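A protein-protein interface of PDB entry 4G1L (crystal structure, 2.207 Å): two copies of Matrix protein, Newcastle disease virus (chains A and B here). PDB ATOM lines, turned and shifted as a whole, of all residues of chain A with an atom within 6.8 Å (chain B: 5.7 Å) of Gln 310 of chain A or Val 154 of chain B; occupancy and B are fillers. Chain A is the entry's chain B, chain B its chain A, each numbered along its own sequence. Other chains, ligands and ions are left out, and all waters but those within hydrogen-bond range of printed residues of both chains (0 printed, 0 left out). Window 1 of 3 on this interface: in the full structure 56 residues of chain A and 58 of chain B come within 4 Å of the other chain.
The side-chain amide oxygen (OE1) of Gln 310 of chain B sits close to the backbone carbonyl oxygen (O) of Lys 158 of chain A. The side-chain carboxylate (OE1) of Glu 161 of chain B sits close to the side-chain amide oxygen (OE1) of Gln 310 of chain A (3.4 Å). The side-chain amide oxygen (OE1) of Gln 310 of chain A sits close to the backbone carbonyl oxygen (O) of Lys 158 of chain B. The side-chain amide nitrogen (NE2) of Gln 310 of chain B sits close to the side-chain amino group (NZ) of Lys 313 of chain A. The side-chain amide nitrogen (NE2) of Gln 310 of chain A sits close to the side-chain amino group (NZ) of Lys 313 of chain B (3.1 Å). N of Glu 125 of chain B lies within hydrogen-bond range of O of Ala 307 of chain A (3.0 Å). The side-chain hydroxyl (OG) of Ser 223 of chain A is in hydrogen-bond range of the side-chain carboxylate (OE2) of Glu 161 of chain B, at 2.8 Å.
The backbone carbonyl oxygen (O) of Val 154 of chain A sits at hydrogen-bond distance from the side-chain amino group (NZ) of Lys 313 of chain A (2.8 Å). O of Lys 158 of chain A lies within hydrogen-bond range of NZ of Lys 313 of chain A, at 2.9 Å. NZ of Lys 313 of chain B lies within hydrogen-bond range of O of Lys 158 of chain B (3.2 Å). OG of Ser 308 of chain A lies within hydrogen-bond range of N of Val 311 of chain A, at 3.4 Å. The backbone carbonyl oxygen (O) of Val 154 of chain B lies within hydrogen-bond range of the side-chain amino group (NZ) of Lys 313 of chain B, at 2.8 Å. The side-chain amide oxygen (OD1) of Asn 152 of chain B sits at hydrogen-bond distance from the backbone NH (N) of Val 154 of chain B, at 2.9 Å.
Among the printed residues, pairs that only touch across the chains: Val 154 of chain A with Gln 310 of chain B (3.9 Å), Ser 223 of chain A with Ala 159 of chain B (3.9 Å), Ser 308 of chain A with Glu 125 of chain B (3.7 Å), Gln 310 of chain A with Val 154 of chain B (3.6 Å), Gln 310 of chain A with Pro 160 of chain B (3.4 Å), Gln 310 of chain A with Gln 310 of chain B (3.99 Å) and Val 311 of chain A with Glu 161 of chain B (3.5 Å).
Of the printed residues of chain B, Ser 308 of chain A touches Glu 125. Printed residues of chain B within 4 Å of Gln 310 of chain A: Val 154, Lys 158, Pro 160, Glu 161, Gln 310 and Lys 313. Printed residues of chain B within 4 Å of Val 311 of chain A: Glu 161 (3.5 Å). Printed residues of chain A within 4 Å of Glu 125 of chain B: Ala 307 and Ser 308. Of chain A, only Gln 310 (3.6 Å) comes within 4 Å of Val 154 of chain B. Of the printed residues of chain A, Ala 159 of chain B touches Ser 223. Of the printed residues of chain A, Pro 160 of chain B touches Gln 310. The nearest printed residue of chain B that does not touch Gln 310 of chain A is Ala 159 of chain B (4.1 Å). The nearest printed residue of chain A that does not touch Lys 158 of chain B is Ser 223 of chain A (6.3 Å).
Of the 14 printed residues of chain A, 8 touch a printed residue of chain B. Printed residues of chain A that touch a printed residue of chain B: Val 154, Lys 158, Ser 223, Ala 307, Ser 308, Gln 310, Val 311 and Lys 313. Along chain A the printed residues that touch a printed residue of chain B span positions 154 to 313.
Val 154 of chain A touches Gln 310 of chain B, and with the chains exchanged Gln 310 of chain A touches Val 154 of chain B. Lys 158 of chain A touches Gln 310 of chain B, and with the chains exchanged Gln 310 of chain A touches Lys 158 of chain B. Gln 310 of chain A touches its own counterpart, Gln 310 of chain B. Gln 310 of chain A touches Lys 313 of chain B, and with the chains exchanged Lys 313 of chain A touches Gln 310 of chain B. Positions printed for both chains: 154, 158, 309, 310 and 313. Of the 14 pairs that touch across the chains among the printed residues, 7 have their exchanged pair printed and touching as well.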
ATOM      1  N   VAL A 154      38.342  10.457  29.421  1.00  0.00           N
ATOM      2  CA  VAL A 154      37.063   9.815  29.140  1.00  0.00           C
ATOM      3  C   VAL A 154      36.406  10.463  27.902  1.00  0.00           C
ATOM      4  O   VAL A 154      35.778   9.752  27.088  1.00  0.00           O
ATOM      5  CB  VAL A 154      36.120   9.827  30.366  1.00  0.00           C
ATOM      6  CG1 VAL A 154      35.519  11.204  30.630  1.00  0.00           C
ATOM      7  CG2 VAL A 154      35.042   8.749  30.216  1.00  0.00           C
ATOM      8  N   LYS A 158      38.407   6.184  23.603  1.00  0.00           N
ATOM      9  CA  LYS A 158      37.191   5.380  23.573  1.00  0.00           C
ATOM     10  C   LYS A 158      37.124   4.588  24.874  1.00  0.00           C
ATOM     11  O   LYS A 158      36.086   4.609  25.573  1.00  0.00           O
ATOM     12  CB  LYS A 158      37.155   4.501  22.341  1.00  0.00           C
ATOM     13  CG  LYS A 158      35.892   3.685  22.167  1.00  0.00           C
ATOM     14  CD  LYS A 158      34.694   4.492  21.676  1.00  0.00           C
ATOM     15  CE  LYS A 158      33.384   3.743  22.004  1.00  0.00           C
ATOM     16  NZ  LYS A 158      32.136   4.274  21.336  1.00  0.00           N
ATOM     17  N   SER A 223      23.625   0.545  23.261  1.00  0.00           N
ATOM     18  CA  SER A 223      23.374   1.738  24.024  1.00  0.00           C
ATOM     19  C   SER A 223      22.497   2.736  23.250  1.00  0.00           C
ATOM     20  O   SER A 223      22.246   3.849  23.712  1.00  0.00           O
ATOM     21  CB  SER A 223      24.684   2.315  24.565  1.00  0.00           C
ATOM     22  OG  SER A 223      25.324   3.123  23.604  1.00  0.00           O
ATOM     23  N   ILE A 304      29.706  18.354  21.929  1.00  0.00           N
ATOM     24  CA  ILE A 304      29.021  17.186  22.524  1.00  0.00           C
ATOM     25  C   ILE A 304      29.848  16.481  23.631  1.00  0.00           C
ATOM     26  O   ILE A 304      29.302  15.989  24.637  1.00  0.00           O
ATOM     27  CB  ILE A 304      28.557  16.223  21.424  1.00  0.00           C
ATOM     28  CG1 ILE A 304      27.754  17.068  20.396  1.00  0.00           C
ATOM     29  CG2 ILE A 304      27.758  15.088  22.065  1.00  0.00           C
ATOM     30  CD1 ILE A 304      27.414  16.429  19.056  1.00  0.00           C
ATOM     31  N   SER A 305      31.166  16.477  23.487  1.00  0.00           N
ATOM     32  CA  SER A 305      31.997  15.762  24.462  1.00  0.00           C
ATOM     33  C   SER A 305      31.925  16.381  25.885  1.00  0.00           C
ATOM     34  O   SER A 305      32.277  15.732  26.866  1.00  0.00           O
ATOM     35  CB  SER A 305      33.436  15.620  23.963  1.00  0.00           C
ATOM     36  OG  SER A 305      34.033  16.890  23.999  1.00  0.00           O
ATOM     37  N   ALA A 307      28.658  17.948  26.854  1.00  0.00           N
ATOM     38  CA  ALA A 307      27.281  17.610  27.132  1.00  0.00           C
ATOM     39  C   ALA A 307      27.149  16.143  27.438  1.00  0.00           C
ATOM     40  O   ALA A 307      26.474  15.786  28.397  1.00  0.00           O
ATOM     41  CB  ALA A 307      26.417  17.966  25.928  1.00  0.00           C
ATOM     42  N   SER A 308      27.790  15.294  26.635  1.00  0.00           N
ATOM     43  CA  SER A 308      27.626  13.840  26.744  1.00  0.00           C
ATOM     44  C   SER A 308      28.811  13.150  26.129  1.00  0.00           C
ATOM     45  O   SER A 308      28.873  13.027  24.901  1.00  0.00           O
ATOM     46  CB  SER A 308      26.344  13.359  26.027  1.00  0.00           C
ATOM     47  OG  SER A 308      26.256  11.927  26.020  1.00  0.00           O
ATOM     48  N   PRO A 309      29.761  12.694  26.974  1.00  0.00           N
ATOM     49  CA  PRO A 309      30.935  12.042  26.400  1.00  0.00           C
ATOM     50  C   PRO A 309      30.601  10.792  25.618  1.00  0.00           C
ATOM     51  O   PRO A 309      31.362  10.415  24.718  1.00  0.00           O
ATOM     52  CB  PRO A 309      31.792  11.695  27.639  1.00  0.00           C
ATOM     53  CG  PRO A 309      31.451  12.790  28.602  1.00  0.00           C
ATOM     54  CD  PRO A 309      29.971  13.022  28.404  1.00  0.00           C
ATOM     55  N   GLN A 310      29.497  10.138  25.949  1.00  0.00           N
ATOM     56  CA  GLN A 310      29.199   8.843  25.299  1.00  0.00           C
ATOM     57  C   GLN A 310      28.645   8.986  23.874  1.00  0.00           C
ATOM     58  O   GLN A 310      29.151   8.345  22.951  1.00  0.00           O
ATOM     59  CB  GLN A 310      28.368   7.900  26.194  1.00  0.00           C
ATOM     60  CG  GLN A 310      29.250   6.839  26.861  1.00  0.00           C
ATOM     61  CD  GLN A 310      28.842   6.485  28.290  1.00  0.00           C
ATOM     62  OE1 GLN A 310      27.647   6.351  28.588  1.00  0.00           O
ATOM     63  NE2 GLN A 310      29.843   6.325  29.188  1.00  0.00           N
ATOM     64  N   VAL A 311      27.675   9.878  23.692  1.00  0.00           N
ATOM     65  CA  VAL A 311      27.218  10.297  22.375  1.00  0.00           C
ATOM     66  C   VAL A 311      28.353  10.902  21.534  1.00  0.00           C
ATOM     67  O   VAL A 311      28.434  10.631  20.356  1.00  0.00           O
ATOM     68  CB  VAL A 311      26.078  11.305  22.494  1.00  0.00           C
ATOM     69  CG1 VAL A 311      25.727  11.912  21.155  1.00  0.00           C
ATOM     70  CG2 VAL A 311      24.846  10.673  23.122  1.00  0.00           C
ATOM     71  N   ALA A 312      29.238  11.691  22.135  1.00  0.00           N
ATOM     72  CA  ALA A 312      30.339  12.281  21.385  1.00  0.00           C
ATOM     73  C   ALA A 312      31.231  11.222  20.729  1.00  0.00           C
ATOM     74  O   ALA A 312      31.608  11.367  19.588  1.00  0.00           O
ATOM     75  CB  ALA A 312      31.172  13.215  22.266  1.00  0.00           C
ATOM     76  N   LYS A 313      31.514  10.127  21.430  1.00  0.00           N
ATOM     77  CA  LYS A 313      32.495   9.170  20.934  1.00  0.00           C
ATOM     78  C   LYS A 313      31.872   8.160  19.939  1.00  0.00           C
ATOM     79  O   LYS A 313      32.540   7.666  18.996  1.00  0.00           O
ATOM     80  CB  LYS A 313      33.202   8.483  22.121  1.00  0.00           C
ATOM     81  CG  LYS A 313      34.016   9.435  23.014  1.00  0.00           C
ATOM     82  CD  LYS A 313      34.895   8.683  24.017  1.00  0.00           C
ATOM     83  CE  LYS A 313      34.152   7.994  25.174  1.00  0.00           C
ATOM     84  NZ  LYS A 313      35.105   7.270  26.111  1.00  0.00           N
ATOM     85  N   ILE A 314      30.580   7.900  20.115  1.00  0.00           N
ATOM     86  CA  ILE A 314      29.788   7.256  19.076  1.00  0.00           C
ATOM     87  C   ILE A 314      29.994   7.973  17.750  1.00  0.00           C
ATOM     88  O   ILE A 314      30.287   7.344  16.718  1.00  0.00           O
ATOM     89  CB  ILE A 314      28.289   7.183  19.484  1.00  0.00           C
ATOM     90  CG1 ILE A 314      28.117   6.030  20.468  1.00  0.00           C
ATOM     91  CG2 ILE A 314      27.366   6.949  18.288  1.00  0.00           C
ATOM     92  CD1 ILE A 314      26.879   6.132  21.343  1.00  0.00           C
ATOM     93  N   LEU A 315      29.896   9.302  17.819  1.00  0.00           N
ATOM     94  CA  LEU A 315      30.015  10.166  16.674  1.00  0.00           C
ATOM     95  C   LEU A 315      31.388  10.194  16.043  1.00  0.00           C
ATOM     96  O   LEU A 315      31.503  10.704  14.974  1.00  0.00           O
ATOM     97  CB  LEU A 315      29.626  11.600  17.042  1.00  0.00           C
ATOM     98  CG  LEU A 315      28.125  11.902  17.224  1.00  0.00           C
ATOM     99  CD1 LEU A 315      27.863  13.392  17.191  1.00  0.00           C
ATOM    100  CD2 LEU A 315      27.301  11.215  16.167  1.00  0.00           C
ATOM    101  N   GLU B 125      24.982  17.194  30.622  1.00  0.00           N
ATOM    102  CA  GLU B 125      23.815  16.416  30.853  1.00  0.00           C
ATOM    103  C   GLU B 125      23.667  15.982  32.316  1.00  0.00           C
ATOM    104  O   GLU B 125      24.603  15.416  32.952  1.00  0.00           O
ATOM    105  CB  GLU B 125      23.857  15.166  29.983  1.00  0.00           C
ATOM    106  CG  GLU B 125      23.230  15.347  28.605  1.00  0.00           C
ATOM    107  CD  GLU B 125      22.830  14.027  27.935  1.00  0.00           C
ATOM    108  OE1 GLU B 125      23.440  12.944  28.208  1.00  0.00           O
ATOM    109  OE2 GLU B 125      21.890  14.078  27.116  1.00  0.00           O
ATOM    110  N   ASN B 152      25.558  14.517  37.447  1.00  0.00           N
ATOM    111  CA  ASN B 152      26.218  14.283  36.134  1.00  0.00           C
ATOM    112  C   ASN B 152      25.726  12.955  35.595  1.00  0.00           C
ATOM    113  O   ASN B 152      25.916  11.947  36.243  1.00  0.00           O
ATOM    114  CB  ASN B 152      27.749  14.281  36.304  1.00  0.00           C
ATOM    115  CG  ASN B 152      28.495  14.001  35.005  1.00  0.00           C
ATOM    116  OD1 ASN B 152      28.235  13.011  34.310  1.00  0.00           O
ATOM    117  ND2 ASN B 152      29.471  14.852  34.694  1.00  0.00           N
ATOM    118  N   ALA B 153      25.079  12.948  34.426  1.00  0.00           N
ATOM    119  CA  ALA B 153      24.426  11.738  33.922  1.00  0.00           C
ATOM    120  C   ALA B 153      25.418  10.688  33.431  1.00  0.00           C
ATOM    121  O   ALA B 153      25.134   9.469  33.452  1.00  0.00           O
ATOM    122  CB  ALA B 153      23.413  12.090  32.809  1.00  0.00           C
ATOM    123  N   VAL B 154      26.579  11.130  32.938  1.00  0.00           N
ATOM    124  CA  VAL B 154      27.557  10.109  32.452  1.00  0.00           C
ATOM    125  C   VAL B 154      28.194   9.309  33.611  1.00  0.00           C
ATOM    126  O   VAL B 154      28.528   8.126  33.457  1.00  0.00           O
ATOM    127  CB  VAL B 154      28.605  10.681  31.477  1.00  0.00           C
ATOM    128  CG1 VAL B 154      29.692  11.460  32.198  1.00  0.00           C
ATOM    129  CG2 VAL B 154      29.181   9.576  30.621  1.00  0.00           C
ATOM    130  N   LYS B 155      28.309   9.938  34.780  1.00  0.00           N
ATOM    131  CA  LYS B 155      28.745   9.210  35.987  1.00  0.00           C
ATOM    132  C   LYS B 155      27.668   8.347  36.652  1.00  0.00           C
ATOM    133  O   LYS B 155      28.032   7.490  37.440  1.00  0.00           O
ATOM    134  CB  LYS B 155      29.301  10.155  37.056  1.00  0.00           C
ATOM    135  CG  LYS B 155      30.470  11.026  36.606  1.00  0.00           C
ATOM    136  CD  LYS B 155      30.641  12.222  37.525  1.00  0.00           C
ATOM    137  CE  LYS B 155      31.969  12.923  37.255  1.00  0.00           C
ATOM    138  NZ  LYS B 155      31.940  14.339  37.754  1.00  0.00           N
ATOM    139  N   HIS B 156      26.376   8.567  36.354  1.00  0.00           N
ATOM    140  CA  HIS B 156      25.310   7.924  37.161  1.00  0.00           C
ATOM    141  C   HIS B 156      24.409   7.043  36.399  1.00  0.00           C
ATOM    142  O   HIS B 156      23.729   6.232  36.979  1.00  0.00           O
ATOM    143  CB  HIS B 156      24.525   8.887  38.007  1.00  0.00           C
ATOM    144  CG  HIS B 156      25.361   9.566  39.054  1.00  0.00           C
ATOM    145  ND1 HIS B 156      25.361   9.185  40.343  1.00  0.00           N
ATOM    146  CD2 HIS B 156      26.277  10.620  38.950  1.00  0.00           C
ATOM    147  CE1 HIS B 156      26.208   9.974  41.035  1.00  0.00           C
ATOM    148  NE2 HIS B 156      26.777  10.844  40.167  1.00  0.00           N
ATOM    149  N   VAL B 157      24.438   7.151  35.083  1.00  0.00           N
ATOM    150  CA  VAL B 157      23.629   6.327  34.264  1.00  0.00           C
ATOM    151  C   VAL B 157      24.546   5.535  33.349  1.00  0.00           C
ATOM    152  O   VAL B 157      25.451   6.085  32.726  1.00  0.00           O
ATOM    153  CB  VAL B 157      22.637   7.228  33.484  1.00  0.00           C
ATOM    154  CG1 VAL B 157      21.663   6.383  32.694  1.00  0.00           C
ATOM    155  CG2 VAL B 157      21.881   8.104  34.476  1.00  0.00           C
ATOM    156  N   LYS B 158      24.276   4.246  33.221  1.00  0.00           N
ATOM    157  CA  LYS B 158      25.116   3.394  32.414  1.00  0.00           C
ATOM    158  C   LYS B 158      25.244   3.896  30.977  1.00  0.00           C
ATOM    159  O   LYS B 158      26.359   3.954  30.419  1.00  0.00           O
ATOM    160  CB  LYS B 158      24.569   1.969  32.430  1.00  0.00           C
ATOM    161  CG  LYS B 158      25.428   1.028  31.626  1.00  0.00           C
ATOM    162  CD  LYS B 158      26.793   0.856  32.237  1.00  0.00           C
ATOM    163  CE  LYS B 158      27.759   0.348  31.190  1.00  0.00           C
ATOM    164  NZ  LYS B 158      28.918  -0.316  31.836  1.00  0.00           N
ATOM    165  N   ALA B 159      24.086   4.260  30.408  1.00  0.00           N
ATOM    166  CA  ALA B 159      23.947   4.704  29.015  1.00  0.00           C
ATOM    167  C   ALA B 159      22.961   5.894  28.838  1.00  0.00           C
ATOM    168  O   ALA B 159      21.765   5.703  28.584  1.00  0.00           O
ATOM    169  CB  ALA B 159      23.585   3.528  28.102  1.00  0.00           C
ATOM    170  N   PRO B 160      23.452   7.132  28.994  1.00  0.00           N
ATOM    171  CA  PRO B 160      22.488   8.253  28.846  1.00  0.00           C
ATOM    172  C   PRO B 160      22.000   8.542  27.407  1.00  0.00           C
ATOM    173  O   PRO B 160      20.931   9.072  27.233  1.00  0.00           O
ATOM    174  CB  PRO B 160      23.229   9.476  29.431  1.00  0.00           C
ATOM    175  CG  PRO B 160      24.646   9.014  29.671  1.00  0.00           C
ATOM    176  CD  PRO B 160      24.696   7.533  29.673  1.00  0.00           C
ATOM    177  N   GLU B 161      22.811   8.275  26.399  1.00  0.00           N
ATOM    178  CA  GLU B 161      22.331   8.313  25.031  1.00  0.00           C
ATOM    179  C   GLU B 161      20.962   7.583  24.873  1.00  0.00           C
ATOM    180  O   GLU B 161      20.253   7.798  23.905  1.00  0.00           O
ATOM    181  CB  GLU B 161      23.386   7.677  24.105  1.00  0.00           C
ATOM    182  CG  GLU B 161      23.777   6.248  24.465  1.00  0.00           C
ATOM    183  CD  GLU B 161      24.912   6.116  25.499  1.00  0.00           C
ATOM    184  OE1 GLU B 161      24.940   6.855  26.512  1.00  0.00           O
ATOM    185  OE2 GLU B 161      25.787   5.242  25.300  1.00  0.00           O
ATOM    186  N   PRO B 309      35.219   7.517  34.894  1.00  0.00           N
ATOM    187  CA  PRO B 309      33.804   7.165  34.965  1.00  0.00           C
ATOM    188  C   PRO B 309      33.455   5.827  34.353  1.00  0.00           C
ATOM    189  O   PRO B 309      32.443   5.237  34.725  1.00  0.00           O
ATOM    190  CB  PRO B 309      33.118   8.283  34.151  1.00  0.00           C
ATOM    191  CG  PRO B 309      34.034   9.452  34.333  1.00  0.00           C
ATOM    192  CD  PRO B 309      35.425   8.854  34.305  1.00  0.00           C
ATOM    193  N   GLN B 310      34.247   5.387  33.387  1.00  0.00           N
ATOM    194  CA  GLN B 310      34.014   4.093  32.738  1.00  0.00           C
ATOM    195  C   GLN B 310      34.396   2.907  33.635  1.00  0.00           C
ATOM    196  O   GLN B 310      33.705   1.878  33.629  1.00  0.00           O
ATOM    197  CB  GLN B 310      34.685   4.042  31.347  1.00  0.00           C
ATOM    198  CG  GLN B 310      34.027   5.031  30.373  1.00  0.00           C
ATOM    199  CD  GLN B 310      34.329   4.788  28.897  1.00  0.00           C
ATOM    200  OE1 GLN B 310      35.224   4.016  28.554  1.00  0.00           O
ATOM    201  NE2 GLN B 310      33.544   5.423  28.015  1.00  0.00           N
ATOM    202  N   LYS B 313      31.694   2.587  36.361  1.00  0.00           N
ATOM    203  CA  LYS B 313      30.431   1.898  35.995  1.00  0.00           C
ATOM    204  C   LYS B 313      30.619   0.411  35.859  1.00  0.00           C
ATOM    205  O   LYS B 313      29.708  -0.346  36.208  1.00  0.00           O
ATOM    206  CB  LYS B 313      29.773   2.516  34.773  1.00  0.00           C
ATOM    207  CG  LYS B 313      29.498   4.010  35.013  1.00  0.00           C
ATOM    208  CD  LYS B 313      28.494   4.592  34.021  1.00  0.00           C
ATOM    209  CE  LYS B 313      29.168   4.807  32.668  1.00  0.00           C
ATOM    210  NZ  LYS B 313      28.423   5.834  31.923  1.00  0.00           N
